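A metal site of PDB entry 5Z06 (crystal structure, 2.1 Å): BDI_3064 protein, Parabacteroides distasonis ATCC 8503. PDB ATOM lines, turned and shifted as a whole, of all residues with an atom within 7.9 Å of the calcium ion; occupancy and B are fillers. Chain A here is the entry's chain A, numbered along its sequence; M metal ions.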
ATOM      1  N   PHE A  11      -0.519 -16.152  -4.944  1.00  0.00           N
ATOM      2  CA  PHE A  11      -1.880 -16.278  -4.467  1.00  0.00           C
ATOM      3  C   PHE A  11      -2.736 -17.020  -5.467  1.00  0.00           C
ATOM      4  O   PHE A  11      -2.759 -16.677  -6.638  1.00  0.00           O
ATOM      5  CB  PHE A  11      -2.480 -14.907  -4.241  1.00  0.00           C
ATOM      6  CG  PHE A  11      -3.859 -14.959  -3.695  1.00  0.00           C
ATOM      7  CD1 PHE A  11      -4.070 -15.116  -2.349  1.00  0.00           C
ATOM      8  CD2 PHE A  11      -4.952 -14.890  -4.543  1.00  0.00           C
ATOM      9  CE1 PHE A  11      -5.343 -15.186  -1.836  1.00  0.00           C
ATOM     10  CE2 PHE A  11      -6.233 -14.964  -4.033  1.00  0.00           C
ATOM     11  CZ  PHE A  11      -6.429 -15.112  -2.680  1.00  0.00           C
ATOM     12  N   GLU A  12      -3.428 -18.037  -4.984  1.00  0.00           N
ATOM     13  CA  GLU A  12      -4.526 -18.653  -5.725  1.00  0.00           C
ATOM     14  C   GLU A  12      -5.843 -18.421  -4.994  1.00  0.00           C
ATOM     15  O   GLU A  12      -6.806 -17.932  -5.584  1.00  0.00           O
ATOM     16  CB  GLU A  12      -4.271 -20.139  -5.871  1.00  0.00           C
ATOM     17  CG  GLU A  12      -5.359 -20.858  -6.628  1.00  0.00           C
ATOM     18  CD  GLU A  12      -4.921 -22.234  -7.056  1.00  0.00           C
ATOM     19  OE1 GLU A  12      -4.691 -23.084  -6.170  1.00  0.00           O
ATOM     20  OE2 GLU A  12      -4.796 -22.436  -8.278  1.00  0.00           O
ATOM     21  N   ASN A  13      -5.878 -18.809  -3.735  1.00  0.00           N
ATOM     22  CA  ASN A  13      -7.064 -18.705  -2.884  1.00  0.00           C
ATOM     23  C   ASN A  13      -6.614 -18.614  -1.444  1.00  0.00           C
ATOM     24  O   ASN A  13      -5.612 -19.209  -1.073  1.00  0.00           O
ATOM     25  CB  ASN A  13      -7.962 -19.950  -3.038  1.00  0.00           C
ATOM     26  CG  ASN A  13      -8.855 -19.875  -4.272  1.00  0.00           C
ATOM     27  OD1 ASN A  13      -9.474 -18.850  -4.532  1.00  0.00           O
ATOM     28  ND2 ASN A  13      -8.939 -20.967  -5.025  1.00  0.00           N
ATOM     29  N   SER A  14      -7.347 -17.859  -0.653  1.00  0.00           N
ATOM     30  CA  SER A  14      -7.138 -17.818   0.788  1.00  0.00           C
ATOM     31  C   SER A  14      -7.987 -18.918   1.372  1.00  0.00           C
ATOM     32  O   SER A  14      -9.195 -18.966   1.101  1.00  0.00           O
ATOM     33  CB  SER A  14      -7.562 -16.485   1.360  1.00  0.00           C
ATOM     34  OG  SER A  14      -7.245 -16.400   2.716  1.00  0.00           O
ATOM     35  N   ALA A  43     -11.583 -11.016  -0.811  1.00  0.00           N
ATOM     36  CA  ALA A  43     -12.900 -10.860  -1.388  1.00  0.00           C
ATOM     37  C   ALA A  43     -13.431 -12.240  -1.736  1.00  0.00           C
ATOM     38  O   ALA A  43     -12.845 -12.927  -2.597  1.00  0.00           O
ATOM     39  CB  ALA A  43     -12.832  -9.992  -2.616  1.00  0.00           C
ATOM     40  N   VAL A  46     -15.905 -12.155  -5.444  1.00  0.00           N
ATOM     41  CA  VAL A  46     -15.332 -12.112  -6.777  1.00  0.00           C
ATOM     42  C   VAL A  46     -14.047 -12.867  -6.778  1.00  0.00           C
ATOM     43  O   VAL A  46     -13.208 -12.744  -5.871  1.00  0.00           O
ATOM     44  CB  VAL A  46     -15.096 -10.680  -7.302  1.00  0.00           C
ATOM     45  CG1 VAL A  46     -16.426  -9.997  -7.620  1.00  0.00           C
ATOM     46  CG2 VAL A  46     -14.247  -9.847  -6.347  1.00  0.00           C
ATOM     47  N   ALA A  47     -13.886 -13.653  -7.820  1.00  0.00           N
ATOM     48  CA  ALA A  47     -12.714 -14.475  -7.968  1.00  0.00           C
ATOM     49  C   ALA A  47     -12.646 -14.939  -9.409  1.00  0.00           C
ATOM     50  O   ALA A  47     -13.693 -15.244 -10.025  1.00  0.00           O
ATOM     51  CB  ALA A  47     -12.795 -15.693  -7.059  1.00  0.00           C
ATOM     52  N   PHE A  48     -11.415 -15.015  -9.914  1.00  0.00           N
ATOM     53  CA  PHE A  48     -11.179 -15.792 -11.109  1.00  0.00           C
ATOM     54  C   PHE A  48     -11.151 -17.294 -10.781  1.00  0.00           C
ATOM     55  O   PHE A  48     -12.016 -18.020 -11.244  1.00  0.00           O
ATOM     56  CB  PHE A  48      -9.904 -15.381 -11.832  1.00  0.00           C
ATOM     57  CG  PHE A  48      -9.776 -16.078 -13.136  1.00  0.00           C
ATOM     58  CD1 PHE A  48     -10.543 -15.629 -14.220  1.00  0.00           C
ATOM     59  CD2 PHE A  48      -9.027 -17.237 -13.259  1.00  0.00           C
ATOM     60  CE1 PHE A  48     -10.510 -16.302 -15.420  1.00  0.00           C
ATOM     61  CE2 PHE A  48      -8.995 -17.910 -14.459  1.00  0.00           C
ATOM     62  CZ  PHE A  48      -9.726 -17.434 -15.545  1.00  0.00           C
ATOM     63  N   THR A  49     -10.155 -17.765 -10.030  1.00  0.00           N
ATOM     64  CA  THR A  49     -10.258 -19.111  -9.444  1.00  0.00           C
ATOM     65  C   THR A  49     -11.162 -18.997  -8.232  1.00  0.00           C
ATOM     66  O   THR A  49     -10.809 -18.297  -7.279  1.00  0.00           O
ATOM     67  CB  THR A  49      -8.948 -19.727  -8.972  1.00  0.00           C
ATOM     68  OG1 THR A  49      -8.227 -18.776  -8.206  1.00  0.00           O
ATOM     69  CG2 THR A  49      -8.156 -20.193 -10.143  1.00  0.00           C
ATOM     70  N   PRO A  50     -12.329 -19.642  -8.293  1.00  0.00           N
ATOM     71  CA  PRO A  50     -13.270 -19.524  -7.234  1.00  0.00           C
ATOM     72  C   PRO A  50     -12.741 -19.958  -5.889  1.00  0.00           C
ATOM     73  O   PRO A  50     -11.745 -20.711  -5.760  1.00  0.00           O
ATOM     74  CB  PRO A  50     -14.397 -20.474  -7.648  1.00  0.00           C
ATOM     75  CG  PRO A  50     -13.748 -21.431  -8.553  1.00  0.00           C
ATOM     76  CD  PRO A  50     -12.829 -20.569  -9.332  1.00  0.00           C
ATOM     77  N   GLY A  51     -13.551 -19.526  -4.936  1.00  0.00           N
ATOM     78  CA  GLY A  51     -13.161 -19.256  -3.620  1.00  0.00           C
ATOM     79  C   GLY A  51     -13.152 -17.742  -3.666  1.00  0.00           C
ATOM     80  O   GLY A  51     -14.173 -17.075  -3.570  1.00  0.00           O
ATOM     81  N   ASN A  52     -11.963 -17.187  -3.835  1.00  0.00           N
ATOM     82  CA  ASN A  52     -11.758 -15.808  -3.479  1.00  0.00           C
ATOM     83  C   ASN A  52     -10.602 -15.183  -4.207  1.00  0.00           C
ATOM     84  O   ASN A  52      -9.843 -15.833  -4.926  1.00  0.00           O
ATOM     85  CB  ASN A  52     -11.626 -15.702  -1.945  1.00  0.00           C
ATOM     86  CG  ASN A  52     -10.545 -16.598  -1.393  1.00  0.00           C
ATOM     87  OD1 ASN A  52      -9.409 -16.565  -1.848  1.00  0.00           O
ATOM     88  ND2 ASN A  52     -10.885 -17.396  -0.391  1.00  0.00           N
ATOM     89  N   SER A  53     -10.499 -13.886  -4.001  1.00  0.00           N
ATOM     90  CA  SER A  53      -9.417 -13.102  -4.532  1.00  0.00           C
ATOM     91  C   SER A  53      -9.002 -12.132  -3.455  1.00  0.00           C
ATOM     92  O   SER A  53      -9.641 -12.056  -2.406  1.00  0.00           O
ATOM     93  CB  SER A  53      -9.908 -12.350  -5.763  1.00  0.00           C
ATOM     94  OG  SER A  53     -10.969 -11.471  -5.428  1.00  0.00           O
ATOM     95  N   LEU A  54      -7.937 -11.408  -3.736  1.00  0.00           N
ATOM     96  CA  LEU A  54      -7.450 -10.402  -2.837  1.00  0.00           C
ATOM     97  C   LEU A  54      -8.002  -9.061  -3.254  1.00  0.00           C
ATOM     98  O   LEU A  54      -8.019  -8.711  -4.443  1.00  0.00           O
ATOM     99  CB  LEU A  54      -5.926 -10.371  -2.850  1.00  0.00           C
ATOM    100  CG  LEU A  54      -5.263 -11.620  -2.288  1.00  0.00           C
ATOM    101  CD1 LEU A  54      -3.765 -11.526  -2.473  1.00  0.00           C
ATOM    102  CD2 LEU A  54      -5.569 -11.760  -0.807  1.00  0.00           C
ATOM    103  N   GLN A  90      -4.553 -12.311 -12.414  1.00  0.00           N
ATOM    104  CA  GLN A  90      -5.870 -11.960 -12.903  1.00  0.00           C
ATOM    105  C   GLN A  90      -6.202 -10.684 -12.140  1.00  0.00           C
ATOM    106  O   GLN A  90      -6.062 -10.640 -10.916  1.00  0.00           O
ATOM    107  CB  GLN A  90      -6.861 -13.072 -12.598  1.00  0.00           C
ATOM    108  CG  GLN A  90      -6.628 -14.320 -13.423  1.00  0.00           C
ATOM    109  CD  GLN A  90      -7.169 -14.245 -14.835  1.00  0.00           C
ATOM    110  OE1 GLN A  90      -7.840 -13.285 -15.213  1.00  0.00           O
ATOM    111  NE2 GLN A  90      -6.895 -15.274 -15.607  1.00  0.00           N
ATOM    112  N   TRP A 132     -12.449 -10.058 -15.310  1.00  0.00           N
ATOM    113  CA  TRP A 132     -11.097 -10.490 -14.988  1.00  0.00           C
ATOM    114  C   TRP A 132     -10.227 -10.316 -16.207  1.00  0.00           C
ATOM    115  O   TRP A 132     -10.577 -10.806 -17.265  1.00  0.00           O
ATOM    116  CB  TRP A 132     -11.085 -11.945 -14.513  1.00  0.00           C
ATOM    117  CG  TRP A 132     -11.677 -12.044 -13.152  1.00  0.00           C
ATOM    118  CD1 TRP A 132     -12.943 -12.432 -12.839  1.00  0.00           C
ATOM    119  CD2 TRP A 132     -11.057 -11.663 -11.938  1.00  0.00           C
ATOM    120  NE1 TRP A 132     -13.129 -12.349 -11.482  1.00  0.00           N
ATOM    121  CE2 TRP A 132     -11.983 -11.878 -10.907  1.00  0.00           C
ATOM    122  CE3 TRP A 132      -9.787 -11.180 -11.612  1.00  0.00           C
ATOM    123  CZ2 TRP A 132     -11.685 -11.641  -9.574  1.00  0.00           C
ATOM    124  CZ3 TRP A 132      -9.495 -10.934 -10.278  1.00  0.00           C
ATOM    125  CH2 TRP A 132     -10.443 -11.174  -9.273  1.00  0.00           C
ATOM    126  N   LEU A 174      -7.240  -8.861  -7.138  1.00  0.00           N
ATOM    127  CA  LEU A 174      -6.109  -9.591  -7.661  1.00  0.00           C
ATOM    128  C   LEU A 174      -6.311 -11.042  -7.300  1.00  0.00           C
ATOM    129  O   LEU A 174      -6.607 -11.375  -6.148  1.00  0.00           O
ATOM    130  CB  LEU A 174      -4.817  -9.098  -7.047  1.00  0.00           C
ATOM    131  CG  LEU A 174      -4.650  -7.576  -7.057  1.00  0.00           C
ATOM    132  CD1 LEU A 174      -3.375  -7.233  -6.307  1.00  0.00           C
ATOM    133  CD2 LEU A 174      -4.613  -7.019  -8.472  1.00  0.00           C
ATOM    134  N   ASP A 175      -6.195 -11.893  -8.302  1.00  0.00           N
ATOM    135  CA  ASP A 175      -6.291 -13.304  -8.140  1.00  0.00           C
ATOM    136  C   ASP A 175      -5.207 -13.996  -8.984  1.00  0.00           C
ATOM    137  O   ASP A 175      -4.655 -13.407  -9.919  1.00  0.00           O
ATOM    138  CB  ASP A 175      -7.693 -13.764  -8.561  1.00  0.00           C
ATOM    139  CG  ASP A 175      -8.110 -15.030  -7.888  1.00  0.00           C
ATOM    140  OD1 ASP A 175      -7.359 -15.557  -7.050  1.00  0.00           O
ATOM    141  OD2 ASP A 175      -9.208 -15.543  -8.188  1.00  0.00           O
ATOM    142  N   ASP A 176      -4.907 -15.232  -8.631  1.00  0.00           N
ATOM    143  CA  ASP A 176      -4.031 -16.098  -9.413  1.00  0.00           C
ATOM    144  C   ASP A 176      -2.699 -15.455  -9.762  1.00  0.00           C
ATOM    145  O   ASP A 176      -2.261 -15.459 -10.907  1.00  0.00           O
ATOM    146  CB  ASP A 176      -4.785 -16.592 -10.609  1.00  0.00           C
ATOM    147  CG  ASP A 176      -6.073 -17.215 -10.195  1.00  0.00           C
ATOM    148  OD1 ASP A 176      -6.032 -18.070  -9.287  1.00  0.00           O
ATOM    149  OD2 ASP A 176      -7.121 -16.824 -10.726  1.00  0.00           O
ATOM    150  N   ILE A 177      -2.080 -14.931  -8.715  1.00  0.00           N
ATOM    151  CA  ILE A 177      -0.798 -14.278  -8.785  1.00  0.00           C
ATOM    152  C   ILE A 177       0.209 -15.390  -8.694  1.00  0.00           C
ATOM    153  O   ILE A 177       0.318 -16.089  -7.683  1.00  0.00           O
ATOM    154  CB  ILE A 177      -0.580 -13.300  -7.639  1.00  0.00           C
ATOM    155  CG1 ILE A 177      -1.780 -12.342  -7.523  1.00  0.00           C
ATOM    156  CG2 ILE A 177       0.708 -12.527  -7.860  1.00  0.00           C
ATOM    157  CD1 ILE A 177      -1.768 -11.465  -6.307  1.00  0.00           C
ATOM    158  N   VAL A 236     -11.259 -24.707  -7.195  1.00  0.00           N
ATOM    159  CA  VAL A 236     -10.310 -25.325  -8.093  1.00  0.00           C
ATOM    160  C   VAL A 236      -9.449 -26.253  -7.282  1.00  0.00           C
ATOM    161  O   VAL A 236      -9.180 -26.008  -6.098  1.00  0.00           O
ATOM    162  CB  VAL A 236      -9.396 -24.333  -8.844  1.00  0.00           C
ATOM    163  CG1 VAL A 236     -10.205 -23.509  -9.826  1.00  0.00           C
ATOM    164  CG2 VAL A 236      -8.588 -23.439  -7.909  1.00  0.00           C
HETATM  165 CA    CA M   1      -8.852 -17.408  -6.411  1.00  0.00          CA
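N of Gln 90 sits at hydrogen-bond distance from O of Asp 175 (2.7 Å). The side-chain amide nitrogen of Asn 13 sits at hydrogen-bond distance from the backbone carbonyl oxygen of Pro 50. OD2 of Asp 175 lies close to N of Phe 48 (2.9 Å). The side-chain amide oxygen (OD1) of Asn 52 sits at hydrogen-bond distance from the backbone NH (N) of Ser 14, 2.7 Å away. N of Thr 49 is in hydrogen-bond range of OD2 of Asp 176 (3.3 Å).
The calcium ion is bound by O of Glu 12 (2.3 Å), O of Thr 49 (2.3 Å), OG1 of Thr 49 (2.3 Å), O of Asn 52 (2.4 Å), OD1 of Asn 13 (2.4 Å), OD1 of Asp 175 (2.5 Å) and OD2 of Asp 175 (2.6 Å). The calcium ion has seven donor atoms within binding distance.
Within 4 Å of the calcium ion: Glu 12, Asn 13, Thr 49, Asn 52 and Asp 175. The nearest printed residue that does not touch the calcium ion is Asp 176 (4.1 Å).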
